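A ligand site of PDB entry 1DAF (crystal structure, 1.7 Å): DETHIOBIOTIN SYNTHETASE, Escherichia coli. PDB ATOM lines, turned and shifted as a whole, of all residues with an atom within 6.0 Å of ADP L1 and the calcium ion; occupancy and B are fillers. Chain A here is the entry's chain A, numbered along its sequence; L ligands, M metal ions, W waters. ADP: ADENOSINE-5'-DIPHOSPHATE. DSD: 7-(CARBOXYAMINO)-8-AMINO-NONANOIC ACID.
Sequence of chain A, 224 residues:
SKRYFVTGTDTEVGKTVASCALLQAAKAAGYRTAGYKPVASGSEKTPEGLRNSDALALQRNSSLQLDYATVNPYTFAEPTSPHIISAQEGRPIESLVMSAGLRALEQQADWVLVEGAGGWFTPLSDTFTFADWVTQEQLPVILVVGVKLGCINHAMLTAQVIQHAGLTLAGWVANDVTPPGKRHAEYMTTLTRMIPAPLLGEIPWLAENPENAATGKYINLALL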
ATOM      1  N   ASP A  10      -8.728   4.793 -23.938  1.00  0.00           N
ATOM      2  CA  ASP A  10      -8.464   4.630 -22.520  1.00  0.00           C
ATOM      3  C   ASP A  10      -9.173   5.771 -21.776  1.00  0.00           C
ATOM      4  O   ASP A  10      -9.799   6.651 -22.386  1.00  0.00           O
ATOM      5  CB  ASP A  10      -6.946   4.730 -22.258  1.00  0.00           C
ATOM      6  CG  ASP A  10      -6.450   4.204 -20.917  1.00  0.00           C
ATOM      7  OD1 ASP A  10      -7.216   3.642 -20.136  1.00  0.00           O
ATOM      8  OD2 ASP A  10      -5.265   4.371 -20.621  1.00  0.00           O
ATOM      9  N   THR A  11      -9.157   5.760 -20.437  1.00  0.00           N
ATOM     10  CA  THR A  11      -9.539   6.887 -19.616  1.00  0.00           C
ATOM     11  C   THR A  11      -8.434   7.966 -19.779  1.00  0.00           C
ATOM     12  O   THR A  11      -7.287   7.638 -20.100  1.00  0.00           O
ATOM     13  CB  THR A  11      -9.673   6.329 -18.159  1.00  0.00           C
ATOM     14  OG1 THR A  11     -10.281   7.360 -17.385  1.00  0.00           O
ATOM     15  CG2 THR A  11      -8.346   5.914 -17.551  1.00  0.00           C
ATOM     16  N   GLU A  12      -8.797   9.250 -19.576  1.00  0.00           N
ATOM     17  CA  GLU A  12      -7.901  10.388 -19.672  1.00  0.00           C
ATOM     18  C   GLU A  12      -7.104  10.487 -20.990  1.00  0.00           C
ATOM     19  O   GLU A  12      -5.901  10.730 -21.046  1.00  0.00           O
ATOM     20  CB  GLU A  12      -6.934  10.380 -18.444  1.00  0.00           C
ATOM     21  CG  GLU A  12      -7.412  11.184 -17.211  1.00  0.00           C
ATOM     22  CD  GLU A  12      -8.589  10.632 -16.382  1.00  0.00           C
ATOM     23  OE1 GLU A  12      -8.678   9.431 -16.115  1.00  0.00           O
ATOM     24  OE2 GLU A  12      -9.425  11.450 -15.978  1.00  0.00           O
ATOM     25  N   VAL A  13      -7.830  10.289 -22.103  1.00  0.00           N
ATOM     26  CA  VAL A  13      -7.232  10.482 -23.425  1.00  0.00           C
ATOM     27  C   VAL A  13      -7.792  11.735 -24.103  1.00  0.00           C
ATOM     28  O   VAL A  13      -7.394  12.050 -25.221  1.00  0.00           O
ATOM     29  CB  VAL A  13      -7.491   9.258 -24.392  1.00  0.00           C
ATOM     30  CG1 VAL A  13      -6.680   8.074 -23.846  1.00  0.00           C
ATOM     31  CG2 VAL A  13      -8.981   8.900 -24.540  1.00  0.00           C
ATOM     32  N   GLY A  14      -8.723  12.472 -23.469  1.00  0.00           N
ATOM     33  CA  GLY A  14      -9.366  13.629 -24.078  1.00  0.00           C
ATOM     34  C   GLY A  14     -10.756  13.345 -24.658  1.00  0.00           C
ATOM     35  O   GLY A  14     -11.188  14.141 -25.494  1.00  0.00           O
ATOM     36  N   LYS A  15     -11.524  12.293 -24.274  1.00  0.00           N
ATOM     37  CA  LYS A  15     -12.909  12.109 -24.718  1.00  0.00           C
ATOM     38  C   LYS A  15     -13.776  13.353 -24.441  1.00  0.00           C
ATOM     39  O   LYS A  15     -14.548  13.749 -25.310  1.00  0.00           O
ATOM     40  CB  LYS A  15     -13.716  10.996 -23.997  1.00  0.00           C
ATOM     41  CG  LYS A  15     -13.520   9.524 -24.270  1.00  0.00           C
ATOM     42  CD  LYS A  15     -14.367   8.645 -23.269  1.00  0.00           C
ATOM     43  CE  LYS A  15     -13.892   8.686 -21.788  1.00  0.00           C
ATOM     44  NZ  LYS A  15     -12.442   8.406 -21.652  1.00  0.00           N
ATOM     45  N   THR A  16     -13.614  13.985 -23.260  1.00  0.00           N
ATOM     46  CA  THR A  16     -14.418  15.166 -22.972  1.00  0.00           C
ATOM     47  C   THR A  16     -13.993  16.352 -23.821  1.00  0.00           C
ATOM     48  O   THR A  16     -14.868  17.045 -24.347  1.00  0.00           O
ATOM     49  CB  THR A  16     -14.301  15.515 -21.480  1.00  0.00           C
ATOM     50  OG1 THR A  16     -14.622  14.324 -20.747  1.00  0.00           O
ATOM     51  CG2 THR A  16     -15.237  16.664 -21.094  1.00  0.00           C
ATOM     52  N   VAL A  17     -12.675  16.543 -24.027  1.00  0.00           N
ATOM     53  CA  VAL A  17     -12.186  17.672 -24.836  1.00  0.00           C
ATOM     54  C   VAL A  17     -12.677  17.495 -26.268  1.00  0.00           C
ATOM     55  O   VAL A  17     -13.233  18.446 -26.830  1.00  0.00           O
ATOM     56  CB  VAL A  17     -10.603  17.744 -24.774  1.00  0.00           C
ATOM     57  CG1 VAL A  17     -10.089  18.724 -25.839  1.00  0.00           C
ATOM     58  CG2 VAL A  17     -10.152  18.201 -23.377  1.00  0.00           C
ATOM     59  N   ALA A  18     -12.579  16.261 -26.802  1.00  0.00           N
ATOM     60  CA  ALA A  18     -13.060  16.033 -28.147  1.00  0.00           C
ATOM     61  C   ALA A  18     -14.592  16.182 -28.264  1.00  0.00           C
ATOM     62  O   ALA A  18     -15.065  16.665 -29.298  1.00  0.00           O
ATOM     63  CB  ALA A  18     -12.649  14.632 -28.592  1.00  0.00           C
ATOM     64  N   LYS A  37     -23.877  12.615 -20.443  1.00  0.00           N
ATOM     65  CA  LYS A  37     -22.877  11.733 -19.854  1.00  0.00           C
ATOM     66  C   LYS A  37     -23.718  10.953 -18.829  1.00  0.00           C
ATOM     67  O   LYS A  37     -23.881  11.438 -17.719  1.00  0.00           O
ATOM     68  CB  LYS A  37     -21.770  12.559 -19.156  1.00  0.00           C
ATOM     69  CG  LYS A  37     -20.578  11.611 -18.868  1.00  0.00           C
ATOM     70  CD  LYS A  37     -19.376  12.280 -18.263  1.00  0.00           C
ATOM     71  CE  LYS A  37     -18.378  11.263 -17.623  1.00  0.00           C
ATOM     72  NZ  LYS A  37     -17.513  10.616 -18.596  1.00  0.00           N
ATOM     73  N   SER A  53     -16.932  17.440 -13.343  1.00  0.00           N
ATOM     74  CA  SER A  53     -16.363  18.427 -14.247  1.00  0.00           C
ATOM     75  C   SER A  53     -16.578  18.130 -15.723  1.00  0.00           C
ATOM     76  O   SER A  53     -16.830  19.046 -16.513  1.00  0.00           O
ATOM     77  CB  SER A  53     -14.848  18.567 -13.994  1.00  0.00           C
ATOM     78  OG  SER A  53     -14.233  17.329 -14.358  1.00  0.00           O
ATOM     79  N   ASP A  54     -16.563  16.829 -16.129  1.00  0.00           N
ATOM     80  CA  ASP A  54     -16.786  16.480 -17.533  1.00  0.00           C
ATOM     81  C   ASP A  54     -18.238  16.695 -17.979  1.00  0.00           C
ATOM     82  O   ASP A  54     -18.503  17.364 -19.001  1.00  0.00           O
ATOM     83  CB  ASP A  54     -16.343  15.024 -17.778  1.00  0.00           C
ATOM     84  CG  ASP A  54     -14.821  14.811 -17.647  1.00  0.00           C
ATOM     85  OD1 ASP A  54     -14.002  15.730 -17.662  1.00  0.00           O
ATOM     86  OD2 ASP A  54     -14.462  13.661 -17.540  1.00  0.00           O
ATOM     87  N   GLU A 115     -21.602  10.605 -24.149  1.00  0.00           N
ATOM     88  CA  GLU A 115     -20.208  10.360 -23.794  1.00  0.00           C
ATOM     89  C   GLU A 115     -20.162   9.217 -22.783  1.00  0.00           C
ATOM     90  O   GLU A 115     -20.923   9.261 -21.805  1.00  0.00           O
ATOM     91  CB  GLU A 115     -19.607  11.610 -23.167  1.00  0.00           C
ATOM     92  CG  GLU A 115     -18.119  11.503 -22.999  1.00  0.00           C
ATOM     93  CD  GLU A 115     -17.427  12.614 -22.240  1.00  0.00           C
ATOM     94  OE1 GLU A 115     -17.938  13.718 -22.137  1.00  0.00           O
ATOM     95  OE2 GLU A 115     -16.330  12.381 -21.749  1.00  0.00           O
ATOM     96  N   GLY A 118     -14.674   6.123 -19.051  1.00  0.00           N
ATOM     97  CA  GLY A 118     -13.554   5.240 -19.383  1.00  0.00           C
ATOM     98  C   GLY A 118     -13.550   4.800 -20.852  1.00  0.00           C
ATOM     99  O   GLY A 118     -13.909   5.576 -21.720  1.00  0.00           O
ATOM    100  N   ASN A 175      -6.459  13.181 -30.824  1.00  0.00           N
ATOM    101  CA  ASN A 175      -6.291  14.215 -29.834  1.00  0.00           C
ATOM    102  C   ASN A 175      -4.846  14.289 -29.338  1.00  0.00           C
ATOM    103  O   ASN A 175      -4.294  13.273 -28.899  1.00  0.00           O
ATOM    104  CB  ASN A 175      -7.259  13.932 -28.682  1.00  0.00           C
ATOM    105  CG  ASN A 175      -7.213  15.028 -27.624  1.00  0.00           C
ATOM    106  OD1 ASN A 175      -7.114  16.206 -27.930  1.00  0.00           O
ATOM    107  ND2 ASN A 175      -7.206  14.742 -26.337  1.00  0.00           N
ATOM    108  N   ASP A 176      -4.195  15.451 -29.419  1.00  0.00           N
ATOM    109  CA  ASP A 176      -2.814  15.541 -29.043  1.00  0.00           C
ATOM    110  C   ASP A 176      -2.647  15.890 -27.584  1.00  0.00           C
ATOM    111  O   ASP A 176      -2.721  17.028 -27.143  1.00  0.00           O
ATOM    112  CB  ASP A 176      -2.111  16.590 -29.899  1.00  0.00           C
ATOM    113  CG  ASP A 176      -2.230  16.351 -31.409  1.00  0.00           C
ATOM    114  OD1 ASP A 176      -2.543  15.256 -31.863  1.00  0.00           O
ATOM    115  OD2 ASP A 176      -2.004  17.299 -32.145  1.00  0.00           O
ATOM    116  N   VAL A 177      -2.493  14.829 -26.800  1.00  0.00           N
ATOM    117  CA  VAL A 177      -2.364  14.977 -25.356  1.00  0.00           C
ATOM    118  C   VAL A 177      -0.996  15.507 -24.883  1.00  0.00           C
ATOM    119  O   VAL A 177      -0.890  16.121 -23.809  1.00  0.00           O
ATOM    120  CB  VAL A 177      -2.699  13.592 -24.692  1.00  0.00           C
ATOM    121  CG1 VAL A 177      -4.196  13.402 -24.830  1.00  0.00           C
ATOM    122  CG2 VAL A 177      -1.940  12.428 -25.347  1.00  0.00           C
ATOM    123  N   ILE A 203      -7.209  17.500 -32.761  1.00  0.00           N
ATOM    124  CA  ILE A 203      -7.163  18.595 -31.814  1.00  0.00           C
ATOM    125  C   ILE A 203      -5.738  18.720 -31.321  1.00  0.00           C
ATOM    126  O   ILE A 203      -5.108  17.735 -30.962  1.00  0.00           O
ATOM    127  CB  ILE A 203      -8.130  18.319 -30.633  1.00  0.00           C
ATOM    128  CG1 ILE A 203      -9.535  18.388 -31.231  1.00  0.00           C
ATOM    129  CG2 ILE A 203      -8.021  19.329 -29.480  1.00  0.00           C
ATOM    130  CD1 ILE A 203     -10.420  17.259 -30.692  1.00  0.00           C
ATOM    131  N   PRO A 204      -5.143  19.927 -31.400  1.00  0.00           N
ATOM    132  CA  PRO A 204      -3.762  20.145 -30.993  1.00  0.00           C
ATOM    133  C   PRO A 204      -3.549  20.157 -29.489  1.00  0.00           C
ATOM    134  O   PRO A 204      -4.524  20.297 -28.726  1.00  0.00           O
ATOM    135  CB  PRO A 204      -3.415  21.479 -31.680  1.00  0.00           C
ATOM    136  CG  PRO A 204      -4.713  22.242 -31.656  1.00  0.00           C
ATOM    137  CD  PRO A 204      -5.731  21.154 -31.962  1.00  0.00           C
ATOM    138  N   TRP A 205      -2.286  20.071 -29.045  1.00  0.00           N
ATOM    139  CA  TRP A 205      -1.993  20.225 -27.627  1.00  0.00           C
ATOM    140  C   TRP A 205      -2.311  21.672 -27.236  1.00  0.00           C
ATOM    141  O   TRP A 205      -1.774  22.615 -27.815  1.00  0.00           O
ATOM    142  CB  TRP A 205      -0.482  19.877 -27.359  1.00  0.00           C
ATOM    143  CG  TRP A 205      -0.031  20.125 -25.916  1.00  0.00           C
ATOM    144  CD1 TRP A 205      -0.513  19.358 -24.878  1.00  0.00           C
ATOM    145  CD2 TRP A 205       0.843  21.104 -25.482  1.00  0.00           C
ATOM    146  NE1 TRP A 205       0.032  19.854 -23.790  1.00  0.00           N
ATOM    147  CE2 TRP A 205       0.837  20.881 -24.089  1.00  0.00           C
ATOM    148  CE3 TRP A 205       1.637  22.136 -26.016  1.00  0.00           C
ATOM    149  CZ2 TRP A 205       1.608  21.676 -23.217  1.00  0.00           C
ATOM    150  CZ3 TRP A 205       2.415  22.948 -25.155  1.00  0.00           C
ATOM    151  CH2 TRP A 205       2.408  22.719 -23.754  1.00  0.00           C
ATOM    152  N   LEU A 206      -3.220  21.838 -26.273  1.00  0.00           N
ATOM    153  CA  LEU A 206      -3.631  23.146 -25.808  1.00  0.00           C
ATOM    154  C   LEU A 206      -3.435  23.173 -24.308  1.00  0.00           C
ATOM    155  O   LEU A 206      -4.297  22.727 -23.551  1.00  0.00           O
ATOM    156  CB  LEU A 206      -5.104  23.382 -26.166  1.00  0.00           C
ATOM    157  CG  LEU A 206      -5.388  23.467 -27.657  1.00  0.00           C
ATOM    158  CD1 LEU A 206      -6.811  23.093 -27.909  1.00  0.00           C
ATOM    159  CD2 LEU A 206      -5.043  24.859 -28.152  1.00  0.00           C
ATOM    160  N   ALA A 207      -2.288  23.643 -23.855  1.00  0.00           N
ATOM    161  CA  ALA A 207      -1.940  23.769 -22.439  1.00  0.00           C
ATOM    162  C   ALA A 207      -3.022  24.327 -21.493  1.00  0.00           C
ATOM    163  O   ALA A 207      -3.335  23.760 -20.438  1.00  0.00           O
ATOM    164  CB  ALA A 207      -0.729  24.658 -22.331  1.00  0.00           C
ATOM    165  N   ASN A 209      -6.462  24.957 -20.556  1.00  0.00           N
ATOM    166  CA  ASN A 209      -7.905  24.681 -20.439  1.00  0.00           C
ATOM    167  C   ASN A 209      -8.750  24.319 -21.663  1.00  0.00           C
ATOM    168  O   ASN A 209      -9.808  24.917 -21.944  1.00  0.00           O
ATOM    169  CB  ASN A 209      -8.573  25.885 -19.757  1.00  0.00           C
ATOM    170  CG  ASN A 209      -8.345  25.881 -18.251  1.00  0.00           C
ATOM    171  OD1 ASN A 209      -7.346  25.382 -17.692  1.00  0.00           O
ATOM    172  ND2 ASN A 209      -9.275  26.474 -17.537  1.00  0.00           N
ATOM    173  N   PRO A 210      -8.431  23.203 -22.321  1.00  0.00           N
ATOM    174  CA  PRO A 210      -8.910  22.894 -23.663  1.00  0.00           C
ATOM    175  C   PRO A 210     -10.414  22.622 -23.750  1.00  0.00           C
ATOM    176  O   PRO A 210     -10.965  22.479 -24.828  1.00  0.00           O
ATOM    177  CB  PRO A 210      -8.003  21.730 -24.039  1.00  0.00           C
ATOM    178  CG  PRO A 210      -7.762  20.977 -22.744  1.00  0.00           C
ATOM    179  CD  PRO A 210      -7.664  22.084 -21.733  1.00  0.00           C
ATOM    180  N   GLU A 211     -11.123  22.590 -22.621  1.00  0.00           N
ATOM    181  CA  GLU A 211     -12.571  22.400 -22.604  1.00  0.00           C
ATOM    182  C   GLU A 211     -13.282  23.718 -22.965  1.00  0.00           C
ATOM    183  O   GLU A 211     -14.409  23.715 -23.459  1.00  0.00           O
ATOM    184  CB  GLU A 211     -13.084  21.991 -21.219  1.00  0.00           C
ATOM    185  CG  GLU A 211     -12.398  20.857 -20.477  1.00  0.00           C
ATOM    186  CD  GLU A 211     -10.988  21.155 -19.934  1.00  0.00           C
ATOM    187  OE1 GLU A 211     -10.711  22.310 -19.590  1.00  0.00           O
ATOM    188  OE2 GLU A 211     -10.160  20.216 -19.830  1.00  0.00           O
HETATM  189  PB  ADP L   1     -11.382  11.652 -20.741  1.00  0.00           P
HETATM  190  O1B ADP L   1     -10.963  10.761 -21.845  1.00  0.00           O
HETATM  191  O2B ADP L   1     -12.849  12.203 -20.979  1.00  0.00           O
HETATM  192  O3B ADP L   1     -11.303  10.962 -19.432  1.00  0.00           O
HETATM  193  PA  ADP L   1     -10.421  14.430 -20.583  1.00  0.00           P
HETATM  194  O1A ADP L   1     -11.086  14.735 -19.326  1.00  0.00           O
HETATM  195  O2A ADP L   1     -11.118  14.980 -21.767  1.00  0.00           O
HETATM  196  O3A ADP L   1     -10.342  12.846 -20.752  1.00  0.00           O
HETATM  197  O5' ADP L   1      -8.919  14.929 -20.579  1.00  0.00           O
HETATM  198  C5' ADP L   1      -8.040  14.376 -19.575  1.00  0.00           C
HETATM  199  C4' ADP L   1      -6.972  15.383 -19.222  1.00  0.00           C
HETATM  200  O4' ADP L   1      -6.113  15.572 -20.356  1.00  0.00           O
HETATM  201  C3' ADP L   1      -7.573  16.722 -18.845  1.00  0.00           C
HETATM  202  O3' ADP L   1      -6.831  17.235 -17.734  1.00  0.00           O
HETATM  203  C2' ADP L   1      -7.371  17.566 -20.083  1.00  0.00           C
HETATM  204  O2' ADP L   1      -7.244  18.988 -19.834  1.00  0.00           O
HETATM  205  C1' ADP L   1      -6.110  16.983 -20.714  1.00  0.00           C
HETATM  206  N9  ADP L   1      -6.130  17.087 -22.198  1.00  0.00           N
HETATM  207  C8  ADP L   1      -6.950  16.362 -23.012  1.00  0.00           C
HETATM  208  N7  ADP L   1      -6.806  16.817 -24.244  1.00  0.00           N
HETATM  209  C5  ADP L   1      -5.924  17.796 -24.245  1.00  0.00           C
HETATM  210  C6  ADP L   1      -5.394  18.615 -25.227  1.00  0.00           C
HETATM  211  N6  ADP L   1      -5.727  18.474 -26.491  1.00  0.00           N
HETATM  212  N1  ADP L   1      -4.458  19.549 -24.894  1.00  0.00           N
HETATM  213  C2  ADP L   1      -4.057  19.669 -23.601  1.00  0.00           C
HETATM  214  N3  ADP L   1      -4.558  18.894 -22.646  1.00  0.00           N
HETATM  215  C4  ADP L   1      -5.481  17.955 -22.931  1.00  0.00           C
HETATM  216  C1  DSD L   2     -11.427   0.206 -16.268  1.00  0.00           C
HETATM  217  O1  DSD L   2     -10.535  -0.149 -15.478  1.00  0.00           O
HETATM  218  O2  DSD L   2     -11.406  -0.110 -17.456  1.00  0.00           O
HETATM  219  C2  DSD L   2     -12.573   1.098 -15.807  1.00  0.00           C
HETATM  220  C3  DSD L   2     -12.146   2.554 -15.698  1.00  0.00           C
HETATM  221  C4  DSD L   2     -13.251   3.486 -15.253  1.00  0.00           C
HETATM  222  C5  DSD L   2     -12.807   4.913 -15.537  1.00  0.00           C
HETATM  223  C6  DSD L   2     -13.855   5.893 -15.038  1.00  0.00           C
HETATM  224  C7  DSD L   2     -13.737   7.346 -15.490  1.00  0.00           C
HETATM  225  C8  DSD L   2     -12.518   8.040 -14.839  1.00  0.00           C
HETATM  226  C9  DSD L   2     -12.640   8.083 -13.314  1.00  0.00           C
HETATM  227  N7  DSD L   2     -14.979   8.012 -15.107  1.00  0.00           N
HETATM  228  C   DSD L   2     -15.645   8.851 -15.926  1.00  0.00           C
HETATM  229  O   DSD L   2     -15.395   8.894 -17.124  1.00  0.00           O
HETATM  230  OXT DSD L   2     -16.542   9.540 -15.436  1.00  0.00           O
HETATM  231  N8  DSD L   2     -12.485   9.397 -15.384  1.00  0.00           N
HETATM  232 CA    CA M   1     -11.869  14.588 -17.145  1.00  0.00          CA
HETATM  233  O   HOH W   1     -14.734  11.527 -19.189  1.00  0.00           O
HETATM  234  O   HOH W   2      -9.371  14.530 -16.139  1.00  0.00           O
HETATM  235  O   HOH W   3     -12.915   8.715 -18.638  1.00  0.00           O
HETATM  236  O   HOH W   4     -12.545  15.029 -14.719  1.00  0.00           O
HETATM  237  O   HOH W   5     -11.618  17.589 -20.058  1.00  0.00           O
HETATM  238  O   HOH W   6     -11.058  16.908 -16.955  1.00  0.00           O
HETATM  239  O   HOH W   7     -11.993  12.394 -17.288  1.00  0.00           O
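Water W7 bridges O3B of ADP L1 (2.7 Å) and OE2 of Glu 12 (3.0 Å).
Water W1 lies within hydrogen-bond range of O2B of ADP L1, NZ of Lys 37, OE2 of Glu 115, OG1 of Thr 16 and O of DSD L2.
Water W3 lies within hydrogen-bond range of O3B of ADP L1 (2.9 Å), O of DSD L2 (2.9 Å), NZ of Lys 15 (3.1 Å), N of Gly 118 (3.2 Å) and OG1 of Thr 11 (3.2 Å).
Water W5 bridges OE2 of Glu 211 (3.0 Å) and O2A of ADP L1 (3.2 Å).
The calcium ion is bound by water W7 (2.2 Å), an oxygen (O1A) of ADP L1 (2.3 Å), water W6 (2.5 Å), the side-chain carboxylate (OD1) of Asp 54 (2.5 Å), water W4 (2.6 Å), water W2 (2.7 Å) and the side-chain carboxylate (OD2) of Asp 54 (2.8 Å).
One residue has an atom within 4 Å of the calcium ion: Asp 54.
The side-chain hydroxyl of Thr 16 is in hydrogen-bond range of an oxygen (O2B) of ADP L1 (2.8 Å).
A nitrogen (N8) of DSD L2 is in salt-bridge range of the side-chain carboxylate (OE2) of Glu 12, at 3.7 Å.
A nitrogen (N6) of ADP L1 is in hydrogen-bond range of the backbone carbonyl oxygen (O) of Pro 204, at 3.1 Å.
The backbone NH (N) of Leu 206 is in hydrogen-bond range of a nitrogen (N1) of ADP L1 (2.9 Å).
A nitrogen (N6) of ADP L1 lies within hydrogen-bond range of the backbone carbonyl oxygen (O) of Asp 176, 3.4 Å away.
OE2 of Glu 211 lies within hydrogen-bond range of O2' of ADP L1 (3.2 Å).
The backbone NH of Gly 14 is in hydrogen-bond range of an oxygen (O3A) of ADP L1 (3.2 Å).
The side-chain amino group (NZ) of Lys 15 lies within salt-bridge range of an oxygen (O1B) of ADP L1 (2.8 Å).
An oxygen (O3B) of ADP L1 is in hydrogen-bond range of the backbone NH (N) of Glu 12 (3.0 Å).
O1B of ADP L1 sits at hydrogen-bond distance from N of Lys 15 (2.9 Å).
An oxygen (O) of DSD L2 is in hydrogen-bond range of the backbone NH (N) of Gly 118, at 3.5 Å.
O of DSD L2 is in salt-bridge range of NZ of Lys 37 (3.1 Å).
The side-chain amide nitrogen (ND2) of Asn 175 lies within hydrogen-bond range of a nitrogen (N7) of ADP L1 (3.0 Å).
An oxygen (O2A) of ADP L1 lies within hydrogen-bond range of the backbone NH (N) of Val 17 (3.2 Å).
An oxygen (O2B) of ADP L1 sits at hydrogen-bond distance from the backbone NH (N) of Thr 16 (3.0 Å).
The backbone NH of Val 13 lies within hydrogen-bond range of an oxygen (O1B) of ADP L1.
Residues that only touch ADP L1: Pro 210 (3.6 Å), Glu 115 (3.6 Å), Trp 205 (3.7 Å) and Ile 203 (3.9 Å).
Of the 25 residues printed, 16 come within 4 Å of ADP L1.
Along chain A the residues within 4 Å of ADP L1 span positions 12 to 211.
The side-chain hydroxyl (OG1) of Thr 16 is in hydrogen-bond range of the side-chain carboxylate (OE2) of Glu 115 (2.8 Å).
OG1 of Thr 16 lies close to OD2 of Asp 54.
The backbone carbonyl oxygen (O) of Val 13 is in hydrogen-bond range of the side-chain amide nitrogen (ND2) of Asn 175 (2.9 Å).
The side-chain amino group of Lys 37 is in salt-bridge range of the side-chain carboxylate of Glu 115 (3.8 Å).
O of Asp 10 is in hydrogen-bond range of NZ of Lys 15 (3.3 Å).
The backbone carbonyl oxygen (O) of Gly 118 sits close to the side-chain amino group (NZ) of Lys 15 (3.2 Å).
OG1 of Thr 11 is in hydrogen-bond range of OE1 of Glu 12, 2.9 Å away.
The backbone NH (N) of Asp 176 lies within hydrogen-bond range of the backbone carbonyl oxygen (O) of Ile 203 (2.9 Å).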
